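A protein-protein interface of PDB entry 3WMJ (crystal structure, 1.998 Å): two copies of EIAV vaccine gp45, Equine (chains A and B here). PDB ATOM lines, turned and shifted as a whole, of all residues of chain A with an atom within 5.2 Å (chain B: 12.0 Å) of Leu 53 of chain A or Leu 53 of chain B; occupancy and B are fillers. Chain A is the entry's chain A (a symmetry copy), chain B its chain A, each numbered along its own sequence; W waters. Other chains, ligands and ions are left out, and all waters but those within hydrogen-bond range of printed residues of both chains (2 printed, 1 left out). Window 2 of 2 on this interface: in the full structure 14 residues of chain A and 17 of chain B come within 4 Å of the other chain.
Among the printed residues, merely in contact across the chains: Gln 57 of chain A with Gln 56 of chain B (3.6 Å), Val 50 of chain A with Asp 49 of chain B (3.7 Å), Val 50 of chain A with Val 50 of chain B (3.8 Å), Leu 53 of chain A with Leu 53 of chain B (3.8 Å) and Val 50 of chain A with Thr 46 of chain B (3.9 Å).
The side-chain amino group (NZ) of Lys 54 of chain A is in salt-bridge range of the side-chain carboxylate (OD2) of Asp 49 of chain B, at 3.6 Å. OE1 of Gln 57 of chain B is in hydrogen-bond range of NE2 of Gln 57 of chain A (3.2 Å).
Water W1 lies within hydrogen-bond range of the side-chain carboxylate (OD1) of Asp 49 of chain B and the side-chain amino group (NZ) of Lys 54 of chain A. Water W2 lies within hydrogen-bond range of OE1 of Gln 57 of chain A (3.2 Å) and OE1 of Gln 57 of chain B (3.2 Å).
Of the 15 printed residues of chain B, 6 touch a printed residue of chain A. Printed residues of chain B that touch a printed residue of chain A: Thr 46, Asp 49, Val 50, Leu 53, Gln 56 and Gln 57. Hydrophobic or aromatic side chains of chain B that line the printed part of chain A: Val 50 and Leu 53. Of the 9 printed residues of chain A, 4 touch a printed residue of chain B. Printed residues of chain A that touch a printed residue of chain B: Val 50, Leu 53, Lys 54 and Gln 57. Hydrophobic or aromatic side chains of chain A within 4 Å of the printed part of chain B: Val 50 and Leu 53.
Val 50 of chain A touches Asp 49 of chain B, but with the chains exchanged Asp 49 of chain A does not touch Val 50 of chain B (7.6 Å). Val 50 of chain B touches its own counterpart, Val 50 of chain A. Lys 54 of chain A touches Asp 49 of chain B, but with the chains exchanged Asp 49 of chain A does not touch Lys 54 of chain B (11.3 Å). Gln 57 of chain A touches Gln 56 of chain B, but with the chains exchanged Gln 56 of chain A does not touch Gln 57 of chain B (7.6 Å). Positions printed for both chains: 49, 50, 51, 52, 53, 54, 55, 56 and 57. Of the 7 pairs that touch across the chains among the printed residues, 3 have their exchanged pair printed and touching as well.
No residue of chain B comes within 4 Å of Asp 49 of chain A. Val 50 of chain A touches three residues of chain B. No residue of chain B comes within 4 Å of Leu 52 of chain A. Of the printed residues of chain B, Leu 53 of chain A touches Leu 53. No residue of chain B comes within 4 Å of Gln 56 of chain A. Printed residues of chain B within 4 Å of Gln 57 of chain A: Gln 56 and Gln 57. Of the printed residues of chain A, Val 50 of chain B touches Val 50. Leu 52 of chain B touches none of the printed residues of chain A. Leu 53 of chain B touches just one residue of chain A: Leu 53. Of the printed residues of chain A, Gln 57 of chain B touches Gln 57 (3.2 Å).
The side-chain amide nitrogen of Gln 45 of chain B sits at hydrogen-bond distance from the side-chain carboxylate of Asp 49 of chain B (3.2 Å).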
ATOM      1  N   ASP A  49     -21.480 -21.889 -27.225  1.00  0.00           N
ATOM      2  CA  ASP A  49     -20.465 -21.961 -26.167  1.00  0.00           C
ATOM      3  C   ASP A  49     -21.069 -22.466 -24.862  1.00  0.00           C
ATOM      4  O   ASP A  49     -20.461 -23.274 -24.143  1.00  0.00           O
ATOM      5  CB  ASP A  49     -19.799 -20.600 -25.926  1.00  0.00           C
ATOM      6  CG  ASP A  49     -18.945 -20.135 -27.109  1.00  0.00           C
ATOM      7  OD1 ASP A  49     -18.496 -20.989 -27.916  1.00  0.00           O
ATOM      8  OD2 ASP A  49     -18.722 -18.902 -27.225  1.00  0.00           O
ATOM      9  N   VAL A  50     -22.259 -21.967 -24.545  1.00  0.00           N
ATOM     10  CA  VAL A  50     -22.945 -22.345 -23.312  1.00  0.00           C
ATOM     11  C   VAL A  50     -23.323 -23.830 -23.338  1.00  0.00           C
ATOM     12  O   VAL A  50     -23.149 -24.535 -22.345  1.00  0.00           O
ATOM     13  CB  VAL A  50     -24.184 -21.465 -23.084  1.00  0.00           C
ATOM     14  CG1 VAL A  50     -25.073 -22.050 -22.004  1.00  0.00           C
ATOM     15  CG2 VAL A  50     -23.748 -20.031 -22.712  1.00  0.00           C
ATOM     16  N   GLN A  51     -23.820 -24.307 -24.479  1.00  0.00           N
ATOM     17  CA  GLN A  51     -24.172 -25.719 -24.629  1.00  0.00           C
ATOM     18  C   GLN A  51     -22.967 -26.625 -24.344  1.00  0.00           C
ATOM     19  O   GLN A  51     -23.086 -27.639 -23.638  1.00  0.00           O
ATOM     20  CB  GLN A  51     -24.720 -25.994 -26.038  1.00  0.00           C
ATOM     21  CG  GLN A  51     -26.046 -25.308 -26.359  1.00  0.00           C
ATOM     22  CD  GLN A  51     -27.120 -25.608 -25.343  1.00  0.00           C
ATOM     23  OE1 GLN A  51     -27.431 -24.780 -24.481  1.00  0.00           O
ATOM     24  NE2 GLN A  51     -27.696 -26.797 -25.431  1.00  0.00           N
ATOM     25  N   LEU A  52     -21.801 -26.251 -24.866  1.00  0.00           N
ATOM     26  CA  LEU A  52     -20.575 -27.031 -24.627  1.00  0.00           C
ATOM     27  C   LEU A  52     -20.228 -27.078 -23.143  1.00  0.00           C
ATOM     28  O   LEU A  52     -19.865 -28.133 -22.594  1.00  0.00           O
ATOM     29  CB  LEU A  52     -19.410 -26.447 -25.438  1.00  0.00           C
ATOM     30  CG  LEU A  52     -18.060 -27.156 -25.287  1.00  0.00           C
ATOM     31  CD1 LEU A  52     -18.131 -28.561 -25.869  1.00  0.00           C
ATOM     32  CD2 LEU A  52     -16.956 -26.358 -25.958  1.00  0.00           C
ATOM     33  N   LEU A  53     -20.360 -25.925 -22.499  1.00  0.00           N
ATOM     34  CA  LEU A  53     -20.118 -25.799 -21.067  1.00  0.00           C
ATOM     35  C   LEU A  53     -21.051 -26.703 -20.263  1.00  0.00           C
ATOM     36  O   LEU A  53     -20.619 -27.367 -19.310  1.00  0.00           O
ATOM     37  CB  LEU A  53     -20.275 -24.336 -20.646  1.00  0.00           C
ATOM     38  CG  LEU A  53     -19.105 -23.464 -21.095  1.00  0.00           C
ATOM     39  CD1 LEU A  53     -19.379 -21.973 -20.853  1.00  0.00           C
ATOM     40  CD2 LEU A  53     -17.873 -23.902 -20.330  1.00  0.00           C
ATOM     41  N   LYS A  54     -22.322 -26.742 -20.651  1.00  0.00           N
ATOM     42  CA  LYS A  54     -23.292 -27.603 -19.983  1.00  0.00           C
ATOM     43  C   LYS A  54     -22.945 -29.092 -20.130  1.00  0.00           C
ATOM     44  O   LYS A  54     -23.120 -29.867 -19.189  1.00  0.00           O
ATOM     45  CB  LYS A  54     -24.710 -27.302 -20.482  1.00  0.00           C
ATOM     46  CG  LYS A  54     -25.146 -25.882 -20.178  1.00  0.00           C
ATOM     47  CD  LYS A  54     -26.653 -25.754 -19.992  1.00  0.00           C
ATOM     48  CE  LYS A  54     -27.420 -25.794 -21.284  1.00  0.00           C
ATOM     49  NZ  LYS A  54     -28.844 -25.402 -21.056  1.00  0.00           N
ATOM     50  N   GLU A  55     -22.437 -29.478 -21.300  1.00  0.00           N
ATOM     51  CA  GLU A  55     -21.974 -30.849 -21.540  1.00  0.00           C
ATOM     52  C   GLU A  55     -20.725 -31.151 -20.716  1.00  0.00           C
ATOM     53  O   GLU A  55     -20.610 -32.218 -20.111  1.00  0.00           O
ATOM     54  CB  GLU A  55     -21.674 -31.062 -23.031  1.00  0.00           C
ATOM     55  CG  GLU A  55     -22.910 -31.119 -23.917  1.00  0.00           C
ATOM     56  CD  GLU A  55     -23.641 -32.448 -23.825  1.00  0.00           C
ATOM     57  OE1 GLU A  55     -23.023 -33.441 -23.377  1.00  0.00           O
ATOM     58  OE2 GLU A  55     -24.829 -32.498 -24.210  1.00  0.00           O
ATOM     59  N   GLN A  56     -19.795 -30.197 -20.690  1.00  0.00           N
ATOM     60  CA  GLN A  56     -18.551 -30.330 -19.936  1.00  0.00           C
ATOM     61  C   GLN A  56     -18.759 -30.393 -18.419  1.00  0.00           C
ATOM     62  O   GLN A  56     -17.803 -30.578 -17.666  1.00  0.00           O
ATOM     63  CB  GLN A  56     -17.604 -29.179 -20.268  1.00  0.00           C
ATOM     64  CG  GLN A  56     -16.963 -29.264 -21.653  1.00  0.00           C
ATOM     65  CD  GLN A  56     -16.230 -27.978 -22.025  1.00  0.00           C
ATOM     66  OE1 GLN A  56     -16.529 -26.903 -21.495  1.00  0.00           O
ATOM     67  NE2 GLN A  56     -15.273 -28.082 -22.936  1.00  0.00           N
ATOM     68  N   GLN A  57     -20.004 -30.241 -17.982  1.00  0.00           N
ATOM     69  CA  GLN A  57     -20.334 -30.248 -16.566  1.00  0.00           C
ATOM     70  C   GLN A  57     -20.826 -31.623 -16.135  1.00  0.00           C
ATOM     71  O   GLN A  57     -21.641 -32.244 -16.821  1.00  0.00           O
ATOM     72  CB  GLN A  57     -21.396 -29.183 -16.283  1.00  0.00           C
ATOM     73  CG  GLN A  57     -21.185 -28.402 -14.994  1.00  0.00           C
ATOM     74  CD  GLN A  57     -19.855 -27.671 -14.962  1.00  0.00           C
ATOM     75  OE1 GLN A  57     -19.239 -27.426 -15.998  1.00  0.00           O
ATOM     76  NE2 GLN A  57     -19.407 -27.314 -13.763  1.00  0.00           N
ATOM     77  N   VAL B  43     -31.590 -13.989 -25.168  1.00  0.00           N
ATOM     78  CA  VAL B  43     -30.580 -13.408 -24.293  1.00  0.00           C
ATOM     79  C   VAL B  43     -30.890 -13.680 -22.818  1.00  0.00           C
ATOM     80  O   VAL B  43     -29.990 -14.003 -22.037  1.00  0.00           O
ATOM     81  CB  VAL B  43     -30.467 -11.879 -24.530  1.00  0.00           C
ATOM     82  CG1 VAL B  43     -29.695 -11.204 -23.399  1.00  0.00           C
ATOM     83  CG2 VAL B  43     -29.801 -11.592 -25.865  1.00  0.00           C
ATOM     84  N   LEU B  44     -32.157 -13.537 -22.433  1.00  0.00           N
ATOM     85  CA  LEU B  44     -32.565 -13.816 -21.060  1.00  0.00           C
ATOM     86  C   LEU B  44     -32.354 -15.295 -20.737  1.00  0.00           C
ATOM     87  O   LEU B  44     -31.900 -15.642 -19.652  1.00  0.00           O
ATOM     88  CB  LEU B  44     -34.032 -13.439 -20.833  1.00  0.00           C
ATOM     89  CG  LEU B  44     -34.375 -11.956 -20.734  1.00  0.00           C
ATOM     90  CD1 LEU B  44     -35.886 -11.773 -20.580  1.00  0.00           C
ATOM     91  CD2 LEU B  44     -33.633 -11.297 -19.585  1.00  0.00           C
ATOM     92  N   GLN B  45     -32.681 -16.165 -21.682  1.00  0.00           N
ATOM     93  CA  GLN B  45     -32.564 -17.603 -21.460  1.00  0.00           C
ATOM     94  C   GLN B  45     -31.105 -18.013 -21.306  1.00  0.00           C
ATOM     95  O   GLN B  45     -30.768 -18.824 -20.432  1.00  0.00           O
ATOM     96  CB  GLN B  45     -33.217 -18.372 -22.610  1.00  0.00           C
ATOM     97  CG  GLN B  45     -32.926 -19.874 -22.592  1.00  0.00           C
ATOM     98  CD  GLN B  45     -33.657 -20.583 -21.472  1.00  0.00           C
ATOM     99  OE1 GLN B  45     -34.833 -20.306 -21.211  1.00  0.00           O
ATOM    100  NE2 GLN B  45     -32.966 -21.505 -20.798  1.00  0.00           N
ATOM    101  N   THR B  46     -30.244 -17.427 -22.137  1.00  0.00           N
ATOM    102  CA  THR B  46     -28.809 -17.695 -22.078  1.00  0.00           C
ATOM    103  C   THR B  46     -28.215 -17.197 -20.768  1.00  0.00           C
ATOM    104  O   THR B  46     -27.349 -17.850 -20.178  1.00  0.00           O
ATOM    105  CB  THR B  46     -28.069 -17.052 -23.264  1.00  0.00           C
ATOM    106  OG1 THR B  46     -28.629 -17.542 -24.489  1.00  0.00           O
ATOM    107  CG2 THR B  46     -26.583 -17.404 -23.229  1.00  0.00           C
ATOM    108  N   HIS B  47     -28.679 -16.038 -20.316  1.00  0.00           N
ATOM    109  CA  HIS B  47     -28.253 -15.502 -19.025  1.00  0.00           C
ATOM    110  C   HIS B  47     -28.600 -16.467 -17.888  1.00  0.00           C
ATOM    111  O   HIS B  47     -27.789 -16.698 -16.992  1.00  0.00           O
ATOM    112  CB  HIS B  47     -28.916 -14.141 -18.778  1.00  0.00           C
ATOM    113  CG  HIS B  47     -28.560 -13.512 -17.462  1.00  0.00           C
ATOM    114  ND1 HIS B  47     -27.306 -13.015 -17.190  1.00  0.00           N
ATOM    115  CD2 HIS B  47     -29.307 -13.276 -16.356  1.00  0.00           C
ATOM    116  CE1 HIS B  47     -27.286 -12.514 -15.967  1.00  0.00           C
ATOM    117  NE2 HIS B  47     -28.490 -12.662 -15.437  1.00  0.00           N
ATOM    118  N   ALA B  48     -29.811 -17.017 -17.913  1.00  0.00           N
ATOM    119  CA  ALA B  48     -30.216 -17.988 -16.895  1.00  0.00           C
ATOM    120  C   ALA B  48     -29.309 -19.218 -16.938  1.00  0.00           C
ATOM    121  O   ALA B  48     -28.914 -19.748 -15.884  1.00  0.00           O
ATOM    122  CB  ALA B  48     -31.670 -18.387 -17.089  1.00  0.00           C
ATOM    123  N   ASP B  49     -28.995 -19.694 -18.144  1.00  0.00           N
ATOM    124  CA  ASP B  49     -28.095 -20.846 -18.264  1.00  0.00           C
ATOM    125  C   ASP B  49     -26.718 -20.527 -17.696  1.00  0.00           C
ATOM    126  O   ASP B  49     -26.095 -21.359 -17.016  1.00  0.00           O
ATOM    127  CB  ASP B  49     -27.951 -21.304 -19.722  1.00  0.00           C
ATOM    128  CG  ASP B  49     -29.244 -21.890 -20.295  1.00  0.00           C
ATOM    129  OD1 ASP B  49     -30.109 -22.356 -19.509  1.00  0.00           O
ATOM    130  OD2 ASP B  49     -29.390 -21.886 -21.545  1.00  0.00           O
ATOM    131  N   VAL B  50     -26.231 -19.329 -17.998  1.00  0.00           N
ATOM    132  CA  VAL B  50     -24.913 -18.898 -17.540  1.00  0.00           C
ATOM    133  C   VAL B  50     -24.887 -18.774 -16.013  1.00  0.00           C
ATOM    134  O   VAL B  50     -23.930 -19.203 -15.369  1.00  0.00           O
ATOM    135  CB  VAL B  50     -24.507 -17.576 -18.208  1.00  0.00           C
ATOM    136  CG1 VAL B  50     -23.310 -16.959 -17.508  1.00  0.00           C
ATOM    137  CG2 VAL B  50     -24.200 -17.814 -19.702  1.00  0.00           C
ATOM    138  N   GLN B  51     -25.945 -18.206 -15.435  1.00  0.00           N
ATOM    139  CA  GLN B  51     -26.045 -18.077 -13.980  1.00  0.00           C
ATOM    140  C   GLN B  51     -25.937 -19.444 -13.293  1.00  0.00           C
ATOM    141  O   GLN B  51     -25.224 -19.598 -12.289  1.00  0.00           O
ATOM    142  CB  GLN B  51     -27.360 -17.387 -13.587  1.00  0.00           C
ATOM    143  CG  GLN B  51     -27.485 -15.933 -14.037  1.00  0.00           C
ATOM    144  CD  GLN B  51     -26.325 -15.080 -13.587  1.00  0.00           C
ATOM    145  OE1 GLN B  51     -25.426 -14.762 -14.372  1.00  0.00           O
ATOM    146  NE2 GLN B  51     -26.331 -14.704 -12.317  1.00  0.00           N
ATOM    147  N   LEU B  52     -26.622 -20.445 -13.843  1.00  0.00           N
ATOM    148  CA  LEU B  52     -26.564 -21.805 -13.282  1.00  0.00           C
ATOM    149  C   LEU B  52     -25.146 -22.362 -13.327  1.00  0.00           C
ATOM    150  O   LEU B  52     -24.656 -22.972 -12.358  1.00  0.00           O
ATOM    151  CB  LEU B  52     -27.534 -22.728 -14.032  1.00  0.00           C
ATOM    152  CG  LEU B  52     -27.580 -24.186 -13.560  1.00  0.00           C
ATOM    153  CD1 LEU B  52     -28.147 -24.267 -12.149  1.00  0.00           C
ATOM    154  CD2 LEU B  52     -28.402 -25.035 -14.514  1.00  0.00           C
ATOM    155  N   LEU B  53     -24.487 -22.133 -14.455  1.00  0.00           N
ATOM    156  CA  LEU B  53     -23.105 -22.554 -14.653  1.00  0.00           C
ATOM    157  C   LEU B  53     -22.176 -21.909 -13.625  1.00  0.00           C
ATOM    158  O   LEU B  53     -21.297 -22.576 -13.063  1.00  0.00           O
ATOM    159  CB  LEU B  53     -22.663 -22.216 -16.079  1.00  0.00           C
ATOM    160  CG  LEU B  53     -23.276 -23.148 -17.122  1.00  0.00           C
ATOM    161  CD1 LEU B  53     -22.994 -22.666 -18.552  1.00  0.00           C
ATOM    162  CD2 LEU B  53     -22.697 -24.532 -16.911  1.00  0.00           C
ATOM    163  N   LYS B  54     -22.377 -20.620 -13.368  1.00  0.00           N
ATOM    164  CA  LYS B  54     -21.577 -19.912 -12.373  1.00  0.00           C
ATOM    165  C   LYS B  54     -21.775 -20.477 -10.959  1.00  0.00           C
ATOM    166  O   LYS B  54     -20.820 -20.571 -10.187  1.00  0.00           O
ATOM    167  CB  LYS B  54     -21.866 -18.408 -12.425  1.00  0.00           C
ATOM    168  CG  LYS B  54     -21.500 -17.788 -13.759  1.00  0.00           C
ATOM    169  CD  LYS B  54     -21.098 -16.323 -13.641  1.00  0.00           C
ATOM    170  CE  LYS B  54     -22.265 -15.397 -13.446  1.00  0.00           C
ATOM    171  NZ  LYS B  54     -21.834 -13.975 -13.601  1.00  0.00           N
ATOM    172  N   GLU B  55     -23.006 -20.871 -10.637  1.00  0.00           N
ATOM    173  CA  GLU B  55     -23.313 -21.518  -9.356  1.00  0.00           C
ATOM    174  C   GLU B  55     -22.679 -22.904  -9.283  1.00  0.00           C
ATOM    175  O   GLU B  55     -22.098 -23.280  -8.264  1.00  0.00           O
ATOM    176  CB  GLU B  55     -24.832 -21.633  -9.162  1.00  0.00           C
ATOM    177  CG  GLU B  55     -25.530 -20.311  -8.881  1.00  0.00           C
ATOM    178  CD  GLU B  55     -25.336 -19.833  -7.452  1.00  0.00           C
ATOM    179  OE1 GLU B  55     -24.983 -20.664  -6.585  1.00  0.00           O
ATOM    180  OE2 GLU B  55     -25.545 -18.626  -7.198  1.00  0.00           O
ATOM    181  N   GLN B  56     -22.785 -23.655 -10.378  1.00  0.00           N
ATOM    182  CA  GLN B  56     -22.219 -24.999 -10.470  1.00  0.00           C
ATOM    183  C   GLN B  56     -20.688 -25.023 -10.408  1.00  0.00           C
ATOM    184  O   GLN B  56     -20.081 -26.093 -10.400  1.00  0.00           O
ATOM    185  CB  GLN B  56     -22.683 -25.683 -11.754  1.00  0.00           C
ATOM    186  CG  GLN B  56     -24.145 -26.125 -11.744  1.00  0.00           C
ATOM    187  CD  GLN B  56     -24.617 -26.573 -13.125  1.00  0.00           C
ATOM    188  OE1 GLN B  56     -24.048 -26.178 -14.148  1.00  0.00           O
ATOM    189  NE2 GLN B  56     -25.657 -27.394 -13.160  1.00  0.00           N
ATOM    190  N   GLN B  57     -20.075 -23.845 -10.362  1.00  0.00           N
ATOM    191  CA  GLN B  57     -18.627 -23.727 -10.333  1.00  0.00           C
ATOM    192  C   GLN B  57     -18.131 -23.537  -8.904  1.00  0.00           C
ATOM    193  O   GLN B  57     -18.693 -22.749  -8.143  1.00  0.00           O
ATOM    194  CB  GLN B  57     -18.192 -22.553 -11.212  1.00  0.00           C
ATOM    195  CG  GLN B  57     -16.945 -22.812 -12.047  1.00  0.00           C
ATOM    196  CD  GLN B  57     -17.105 -23.992 -12.988  1.00  0.00           C
ATOM    197  OE1 GLN B  57     -18.218 -24.404 -13.308  1.00  0.00           O
ATOM    198  NE2 GLN B  57     -15.982 -24.540 -13.441  1.00  0.00           N
HETATM  199  O   HOH W   1     -29.578 -24.334 -17.861  1.00  0.00           O
HETATM  200  O   HOH W   2     -18.734 -24.314 -16.450  1.00  0.00           O
